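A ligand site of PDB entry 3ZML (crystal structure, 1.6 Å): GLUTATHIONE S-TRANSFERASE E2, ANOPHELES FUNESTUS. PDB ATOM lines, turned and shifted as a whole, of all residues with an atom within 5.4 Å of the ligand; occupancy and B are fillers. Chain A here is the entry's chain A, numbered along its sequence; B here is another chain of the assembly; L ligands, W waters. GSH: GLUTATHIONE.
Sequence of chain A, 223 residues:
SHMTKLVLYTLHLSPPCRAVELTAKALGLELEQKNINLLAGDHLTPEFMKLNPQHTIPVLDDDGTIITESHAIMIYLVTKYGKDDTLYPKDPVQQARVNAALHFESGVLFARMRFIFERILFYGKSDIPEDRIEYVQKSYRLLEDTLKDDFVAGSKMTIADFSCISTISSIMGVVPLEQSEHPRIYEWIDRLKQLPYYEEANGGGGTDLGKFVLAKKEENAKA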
ATOM      1  N   SER A  14      -0.148  15.497 -32.647  1.00  0.00           N
ATOM      2  CA  SER A  14       0.168  15.400 -31.181  1.00  0.00           C
ATOM      3  C   SER A  14      -1.072  15.778 -30.300  1.00  0.00           C
ATOM      4  O   SER A  14      -1.678  16.880 -30.441  1.00  0.00           O
ATOM      5  CB  SER A  14       1.287  16.411 -30.871  1.00  0.00           C
ATOM      6  OG  SER A  14       1.386  16.616 -29.394  1.00  0.00           O
ATOM      7  N   PRO A  15      -1.453  14.900 -29.389  1.00  0.00           N
ATOM      8  CA  PRO A  15      -2.579  15.264 -28.577  1.00  0.00           C
ATOM      9  C   PRO A  15      -2.429  16.559 -27.747  1.00  0.00           C
ATOM     10  O   PRO A  15      -3.357  17.364 -27.781  1.00  0.00           O
ATOM     11  CB  PRO A  15      -2.777  14.048 -27.649  1.00  0.00           C
ATOM     12  CG  PRO A  15      -2.210  12.908 -28.386  1.00  0.00           C
ATOM     13  CD  PRO A  15      -1.063  13.493 -29.199  1.00  0.00           C
ATOM     14  N   PRO A  16      -1.343  16.749 -26.993  1.00  0.00           N
ATOM     15  CA  PRO A  16      -1.365  17.983 -26.202  1.00  0.00           C
ATOM     16  C   PRO A  16      -1.302  19.245 -27.065  1.00  0.00           C
ATOM     17  O   PRO A  16      -1.796  20.293 -26.650  1.00  0.00           O
ATOM     18  CB  PRO A  16      -0.091  17.877 -25.320  1.00  0.00           C
ATOM     19  CG  PRO A  16       0.778  16.855 -26.044  1.00  0.00           C
ATOM     20  CD  PRO A  16      -0.224  15.855 -26.613  1.00  0.00           C
ATOM     21  N   LEU A  38       8.062  15.870 -35.595  1.00  0.00           N
ATOM     22  CA  LEU A  38       8.672  14.893 -34.725  1.00  0.00           C
ATOM     23  C   LEU A  38       9.188  13.679 -35.517  1.00  0.00           C
ATOM     24  O   LEU A  38      10.167  13.028 -35.108  1.00  0.00           O
ATOM     25  CB  LEU A  38       7.600  14.388 -33.750  1.00  0.00           C
ATOM     26  CG  LEU A  38       7.031  15.411 -32.776  1.00  0.00           C
ATOM     27  CD1 LEU A  38       6.059  14.720 -31.861  1.00  0.00           C
ATOM     28  CD2 LEU A  38       8.091  16.160 -31.964  1.00  0.00           C
ATOM     29  N   HIS A  43      12.527  18.115 -33.179  1.00  0.00           N
ATOM     30  CA  HIS A  43      12.461  18.507 -31.778  1.00  0.00           C
ATOM     31  C   HIS A  43      13.760  18.203 -31.093  1.00  0.00           C
ATOM     32  O   HIS A  43      13.915  18.580 -29.982  1.00  0.00           O
ATOM     33  CB  HIS A  43      11.344  17.744 -31.047  1.00  0.00           C
ATOM     34  CG  HIS A  43      11.404  16.280 -31.264  1.00  0.00           C
ATOM     35  ND1 HIS A  43      11.356  15.349 -30.256  1.00  0.00           N
ATOM     36  CD2 HIS A  43      11.475  15.591 -32.420  1.00  0.00           C
ATOM     37  CE1 HIS A  43      11.408  14.143 -30.791  1.00  0.00           C
ATOM     38  NE2 HIS A  43      11.500  14.281 -32.101  1.00  0.00           N
ATOM     39  N   LEU A  44      14.644  17.493 -31.802  1.00  0.00           N
ATOM     40  CA  LEU A  44      15.970  17.049 -31.215  1.00  0.00           C
ATOM     41  C   LEU A  44      17.157  17.965 -31.577  1.00  0.00           C
ATOM     42  O   LEU A  44      18.310  17.598 -31.410  1.00  0.00           O
ATOM     43  CB  LEU A  44      16.267  15.553 -31.541  1.00  0.00           C
ATOM     44  CG  LEU A  44      15.118  14.639 -30.995  1.00  0.00           C
ATOM     45  CD1 LEU A  44      15.332  13.152 -31.287  1.00  0.00           C
ATOM     46  CD2 LEU A  44      14.894  14.816 -29.505  1.00  0.00           C
ATOM     47  N   GLN A  54      13.213  19.870 -22.251  1.00  0.00           N
ATOM     48  CA  GLN A  54      12.596  18.547 -22.332  1.00  0.00           C
ATOM     49  C   GLN A  54      12.253  18.105 -23.762  1.00  0.00           C
ATOM     50  O   GLN A  54      11.785  17.001 -23.961  1.00  0.00           O
ATOM     51  CB  GLN A  54      11.346  18.442 -21.464  1.00  0.00           C
ATOM     52  CG  GLN A  54      11.644  18.580 -19.978  1.00  0.00           C
ATOM     53  CD  GLN A  54      10.493  19.183 -19.172  1.00  0.00           C
ATOM     54  OE1 GLN A  54       9.386  19.022 -19.533  1.00  0.00           O
ATOM     55  NE2 GLN A  54      10.813  19.835 -18.069  1.00  0.00           N
ATOM     56  N   HIS A  55      12.585  18.961 -24.691  1.00  0.00           N
ATOM     57  CA  HIS A  55      12.356  18.673 -26.110  1.00  0.00           C
ATOM     58  C   HIS A  55      11.004  18.047 -26.497  1.00  0.00           C
ATOM     59  O   HIS A  55      10.939  17.112 -27.230  1.00  0.00           O
ATOM     60  CB  HIS A  55      13.529  17.907 -26.731  1.00  0.00           C
ATOM     61  CG  HIS A  55      13.877  16.626 -26.058  1.00  0.00           C
ATOM     62  ND1 HIS A  55      13.167  15.476 -26.256  1.00  0.00           N
ATOM     63  CD2 HIS A  55      14.904  16.303 -25.238  1.00  0.00           C
ATOM     64  CE1 HIS A  55      13.714  14.504 -25.552  1.00  0.00           C
ATOM     65  NE2 HIS A  55      14.762  14.976 -24.915  1.00  0.00           N
ATOM     66  N   THR A  56       9.934  18.656 -26.000  1.00  0.00           N
ATOM     67  CA  THR A  56       8.593  18.239 -26.343  1.00  0.00           C
ATOM     68  C   THR A  56       7.751  19.371 -26.900  1.00  0.00           C
ATOM     69  O   THR A  56       7.994  20.502 -26.619  1.00  0.00           O
ATOM     70  CB  THR A  56       7.797  17.643 -25.117  1.00  0.00           C
ATOM     71  OG1 THR A  56       7.579  18.611 -24.088  1.00  0.00           O
ATOM     72  CG2 THR A  56       8.486  16.460 -24.573  1.00  0.00           C
ATOM     73  N   ILE A  57       6.790  18.997 -27.737  1.00  0.00           N
ATOM     74  CA  ILE A  57       5.723  19.967 -28.128  1.00  0.00           C
ATOM     75  C   ILE A  57       4.440  19.649 -27.372  1.00  0.00           C
ATOM     76  O   ILE A  57       4.200  18.460 -27.109  1.00  0.00           O
ATOM     77  CB  ILE A  57       5.504  19.880 -29.668  1.00  0.00           C
ATOM     78  CG1 ILE A  57       5.249  18.392 -30.113  1.00  0.00           C
ATOM     79  CG2 ILE A  57       6.711  20.524 -30.364  1.00  0.00           C
ATOM     80  CD1 ILE A  57       4.954  18.227 -31.620  1.00  0.00           C
ATOM     81  N   PRO A  58       3.563  20.648 -27.167  1.00  0.00           N
ATOM     82  CA  PRO A  58       3.670  22.047 -27.641  1.00  0.00           C
ATOM     83  C   PRO A  58       4.544  22.954 -26.837  1.00  0.00           C
ATOM     84  O   PRO A  58       4.798  22.720 -25.649  1.00  0.00           O
ATOM     85  CB  PRO A  58       2.258  22.538 -27.513  1.00  0.00           C
ATOM     86  CG  PRO A  58       1.727  21.788 -26.296  1.00  0.00           C
ATOM     87  CD  PRO A  58       2.229  20.374 -26.546  1.00  0.00           C
ATOM     88  N   GLU A  69       4.620  23.299 -22.305  1.00  0.00           N
ATOM     89  CA  GLU A  69       3.754  22.292 -21.652  1.00  0.00           C
ATOM     90  C   GLU A  69       2.241  22.591 -21.852  1.00  0.00           C
ATOM     91  O   GLU A  69       1.783  23.654 -21.461  1.00  0.00           O
ATOM     92  CB  GLU A  69       4.170  22.098 -20.157  1.00  0.00           C
ATOM     93  CG  GLU A  69       3.843  20.660 -19.643  1.00  0.00           C
ATOM     94  CD  GLU A  69       2.358  20.454 -19.339  1.00  0.00           C
ATOM     95  OE1 GLU A  69       1.671  21.496 -19.037  1.00  0.00           O
ATOM     96  OE2 GLU A  69       1.930  19.269 -19.436  1.00  0.00           O
ATOM     97  N   SER A  70       1.518  21.633 -22.473  1.00  0.00           N
ATOM     98  CA  SER A  70       0.126  21.996 -22.895  1.00  0.00           C
ATOM     99  C   SER A  70      -0.781  22.510 -21.775  1.00  0.00           C
ATOM    100  O   SER A  70      -1.603  23.413 -22.014  1.00  0.00           O
ATOM    101  CB  SER A  70      -0.580  20.827 -23.606  1.00  0.00           C
ATOM    102  OG  SER A  70      -0.857  19.725 -22.740  1.00  0.00           O
ATOM    103  N   HIS A  71      -0.699  21.882 -20.588  1.00  0.00           N
ATOM    104  CA  HIS A  71      -1.623  22.230 -19.504  1.00  0.00           C
ATOM    105  C   HIS A  71      -1.318  23.605 -18.987  1.00  0.00           C
ATOM    106  O   HIS A  71      -2.256  24.433 -18.759  1.00  0.00           O
ATOM    107  CB  HIS A  71      -1.570  21.142 -18.394  1.00  0.00           C
ATOM    108  CG  HIS A  71      -1.721  19.743 -18.918  1.00  0.00           C
ATOM    109  ND1 HIS A  71      -0.671  19.014 -19.367  1.00  0.00           N
ATOM    110  CD2 HIS A  71      -2.830  18.960 -19.121  1.00  0.00           C
ATOM    111  CE1 HIS A  71      -1.103  17.796 -19.804  1.00  0.00           C
ATOM    112  NE2 HIS A  71      -2.428  17.780 -19.678  1.00  0.00           N
ATOM    113  N   SER A 106      -2.460  14.097 -17.666  1.00  0.00           N
ATOM    114  CA  SER A 106      -1.039  13.941 -17.902  1.00  0.00           C
ATOM    115  C   SER A 106      -0.496  12.651 -17.277  1.00  0.00           C
ATOM    116  O   SER A 106       0.285  11.914 -17.943  1.00  0.00           O
ATOM    117  CB  SER A 106      -0.223  15.219 -17.486  1.00  0.00           C
ATOM    118  OG  SER A 106      -0.412  15.460 -16.123  1.00  0.00           O
ATOM    119  N   PHE A 110      -2.612  10.297 -20.811  1.00  0.00           N
ATOM    120  CA  PHE A 110      -1.547  10.545 -21.779  1.00  0.00           C
ATOM    121  C   PHE A 110      -0.377   9.637 -21.537  1.00  0.00           C
ATOM    122  O   PHE A 110       0.210   9.058 -22.470  1.00  0.00           O
ATOM    123  CB  PHE A 110      -1.154  12.008 -21.823  1.00  0.00           C
ATOM    124  CG  PHE A 110      -0.047  12.308 -22.834  1.00  0.00           C
ATOM    125  CD1 PHE A 110      -0.358  12.537 -24.169  1.00  0.00           C
ATOM    126  CD2 PHE A 110       1.309  12.345 -22.435  1.00  0.00           C
ATOM    127  CE1 PHE A 110       0.645  12.821 -25.104  1.00  0.00           C
ATOM    128  CE2 PHE A 110       2.313  12.665 -23.373  1.00  0.00           C
ATOM    129  CZ  PHE A 110       1.969  12.851 -24.741  1.00  0.00           C
ATOM    130  N   ARG A 114       1.183   7.169 -24.327  1.00  0.00           N
ATOM    131  CA  ARG A 114       2.564   7.248 -24.746  1.00  0.00           C
ATOM    132  C   ARG A 114       3.337   5.943 -24.518  1.00  0.00           C
ATOM    133  O   ARG A 114       4.253   5.620 -25.303  1.00  0.00           O
ATOM    134  CB  ARG A 114       3.256   8.491 -24.154  1.00  0.00           C
ATOM    135  CG  ARG A 114       4.688   8.726 -24.595  1.00  0.00           C
ATOM    136  CD  ARG A 114       5.209  10.084 -24.126  1.00  0.00           C
ATOM    137  NE  ARG A 114       6.677  10.037 -24.292  1.00  0.00           N
ATOM    138  CZ  ARG A 114       7.489  11.098 -24.560  1.00  0.00           C
ATOM    139  NH1 ARG A 114       7.010  12.326 -24.645  1.00  0.00           N
ATOM    140  NH2 ARG A 114       8.813  10.872 -24.694  1.00  0.00           N
ATOM    141  N   GLU A 118       4.927   5.649 -28.176  1.00  0.00           N
ATOM    142  CA  GLU A 118       6.250   6.231 -28.468  1.00  0.00           C
ATOM    143  C   GLU A 118       7.200   5.179 -29.064  1.00  0.00           C
ATOM    144  O   GLU A 118       7.975   5.462 -30.026  1.00  0.00           O
ATOM    145  CB  GLU A 118       6.863   6.882 -27.202  1.00  0.00           C
ATOM    146  CG  GLU A 118       8.357   7.276 -27.367  1.00  0.00           C
ATOM    147  CD  GLU A 118       8.987   7.889 -26.143  1.00  0.00           C
ATOM    148  OE1 GLU A 118       8.500   7.687 -25.041  1.00  0.00           O
ATOM    149  OE2 GLU A 118       9.961   8.619 -26.326  1.00  0.00           O
ATOM    150  N   PHE A 122       8.754   5.827 -32.803  1.00  0.00           N
ATOM    151  CA  PHE A 122      10.119   6.375 -32.860  1.00  0.00           C
ATOM    152  C   PHE A 122      11.202   5.345 -32.677  1.00  0.00           C
ATOM    153  O   PHE A 122      12.363   5.604 -33.082  1.00  0.00           O
ATOM    154  CB  PHE A 122      10.322   7.405 -31.736  1.00  0.00           C
ATOM    155  CG  PHE A 122       9.417   8.579 -31.869  1.00  0.00           C
ATOM    156  CD1 PHE A 122       9.742   9.589 -32.772  1.00  0.00           C
ATOM    157  CD2 PHE A 122       8.261   8.700 -31.092  1.00  0.00           C
ATOM    158  CE1 PHE A 122       8.899  10.705 -32.933  1.00  0.00           C
ATOM    159  CE2 PHE A 122       7.455   9.810 -31.236  1.00  0.00           C
ATOM    160  CZ  PHE A 122       7.737  10.800 -32.174  1.00  0.00           C
ATOM    161  N   HIS B 103       3.274  19.244 -14.077  1.00  0.00           N
ATOM    162  CA  HIS B 103       2.814  18.242 -15.056  1.00  0.00           C
ATOM    163  C   HIS B 103       3.946  17.387 -15.565  1.00  0.00           C
ATOM    164  O   HIS B 103       3.722  16.236 -15.982  1.00  0.00           O
ATOM    165  CB  HIS B 103       2.075  18.868 -16.225  1.00  0.00           C
ATOM    166  CG  HIS B 103       0.669  19.250 -15.869  1.00  0.00           C
ATOM    167  ND1 HIS B 103      -0.363  18.381 -15.952  1.00  0.00           N
ATOM    168  CD2 HIS B 103       0.151  20.423 -15.411  1.00  0.00           C
ATOM    169  CE1 HIS B 103      -1.470  18.941 -15.496  1.00  0.00           C
ATOM    170  NE2 HIS B 103      -1.192  20.236 -15.224  1.00  0.00           N
HETATM  171  N1  GSH L   1       3.154  17.135 -20.608  1.00  0.00           N
HETATM  172  CA1 GSH L   1       3.495  17.474 -22.017  1.00  0.00           C
HETATM  173  C1  GSH L   1       2.402  18.364 -22.548  1.00  0.00           C
HETATM  174  O11 GSH L   1       1.239  18.095 -22.279  1.00  0.00           O
HETATM  175  O12 GSH L   1       2.810  19.345 -23.218  1.00  0.00           O
HETATM  176  CB1 GSH L   1       3.719  16.215 -22.898  1.00  0.00           C
HETATM  177  CG1 GSH L   1       4.308  16.636 -24.259  1.00  0.00           C
HETATM  178  CD1 GSH L   1       4.694  15.426 -25.063  1.00  0.00           C
HETATM  179  OE1 GSH L   1       5.054  14.396 -24.513  1.00  0.00           O
HETATM  180  N2  GSH L   1       4.700  15.579 -26.382  1.00  0.00           N
HETATM  181  CA2 GSH L   1       5.233  14.559 -27.307  1.00  0.00           C
HETATM  182  C2  GSH L   1       6.661  14.931 -27.642  1.00  0.00           C
HETATM  183  O2  GSH L   1       6.927  16.134 -27.859  1.00  0.00           O
HETATM  184  CB2 GSH L   1       4.392  14.427 -28.585  1.00  0.00           C
HETATM  185  SG2 GSH L   1       2.707  13.908 -28.282  1.00  0.00           S
HETATM  186  N3  GSH L   1       7.475  13.928 -27.716  1.00  0.00           N
HETATM  187  CA3 GSH L   1       8.908  14.119 -28.149  1.00  0.00           C
HETATM  188  C3  GSH L   1       9.886  13.809 -27.019  1.00  0.00           C
HETATM  189  O31 GSH L   1      11.114  13.850 -27.224  1.00  0.00           O
HETATM  190  O32 GSH L   1       9.452  13.466 -25.904  1.00  0.00           O
HETATM  191  O   HOH W   1       5.330  20.381 -24.121  1.00  0.00           O
HETATM  192  O   HOH W   2       6.273  10.845 -27.732  1.00  0.00           O
HETATM  193  O   HOH W   3       6.172  13.707 -21.846  1.00  0.00           O
HETATM  194  O   HOH W   4       5.983  17.464 -19.537  1.00  0.00           O
HETATM  195  O   HOH W   5       9.432  10.628 -28.176  1.00  0.00           O
HETATM  196  O   HOH W   6      12.859  11.822 -27.659  1.00  0.00           O
HETATM  197  O   HOH W   7      -0.611  15.437 -21.772  1.00  0.00           O
HETATM  198  O   HOH W   8       1.521  15.090 -20.275  1.00  0.00           O
HETATM  199  O   HOH W   9       4.314  15.537 -18.770  1.00  0.00           O
HETATM  200  O   HOH W  10      10.863  14.267 -23.530  1.00  0.00           O
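O of Pro 58 is in hydrogen-bond range of N of Glu 69 (3.4 Å).
OE2 of Glu 69 sits at hydrogen-bond distance from ND1 of His 71 (2.6 Å).
ND1 of His 71 lies within hydrogen-bond range of ND1 of His 103 of chain B (3.5 Å).
The side-chain hydroxyl of Ser 70 lies within hydrogen-bond range of a ring nitrogen (ND1) of His 71 (3.5 Å).
The guanidinium group (NH2) of Arg 114 lies within salt-bridge range of the side-chain carboxylate (OE2) of Glu 118, 3.0 Å away.
Pro 15 touches the ligand.
CB of Pro 16 touches O11 of the ligand, 3.3 Å away.
Leu 38 touches the ligand.
Thr 56 touches the ligand.
Pro 58 touches the ligand (CD to O12, 3.5 Å).
CE1 of His 71 touches O11 of the ligand, at 3.4 Å.
CE2 of Phe 110 touches OE1 of the ligand, 3.4 Å away.
Along chain A the residues within 4 Å of the ligand span positions 14 to 114.
Water W9 bridges a nitrogen (N1) of the ligand (2.7 Å) and the backbone carbonyl oxygen (O) of His 103 of chain B (2.9 Å).
Water W1 lies within hydrogen-bond range of O of Pro 58 (2.8 Å), OG1 of Thr 56 (2.9 Å) and O12 of the ligand (2.9 Å).
Water W10 bridges an oxygen (O32) of the ligand and the backbone carbonyl oxygen (O) of Gln 54.
Water W3 lies within hydrogen-bond range of OE1 of the ligand and NH1 of Arg 114.
An oxygen (O31) of the ligand sits at hydrogen-bond distance from a ring nitrogen (ND1) of His 43 (3.4 Å).
The side-chain hydroxyl (OG) of Ser 14 sits close to a sulfur (SG2) of the ligand (3.2 Å).
N2 of the ligand sits at hydrogen-bond distance from O of Ile 57, 3.0 Å away.
The side-chain carboxylate of Glu 69 is in salt-bridge range of a nitrogen (N1) of the ligand, 2.7 Å away.
OG of Ser 70 sits at hydrogen-bond distance from O11 of the ligand.
O2 of the ligand sits at hydrogen-bond distance from N of Ile 57.
O12 of the ligand is in hydrogen-bond range of N of Ser 70 (2.7 Å).
O32 of the ligand is in salt-bridge range of NH2 of Arg 114, 2.9 Å away.
ND1 of His 55 is in hydrogen-bond range of O31 of the ligand.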
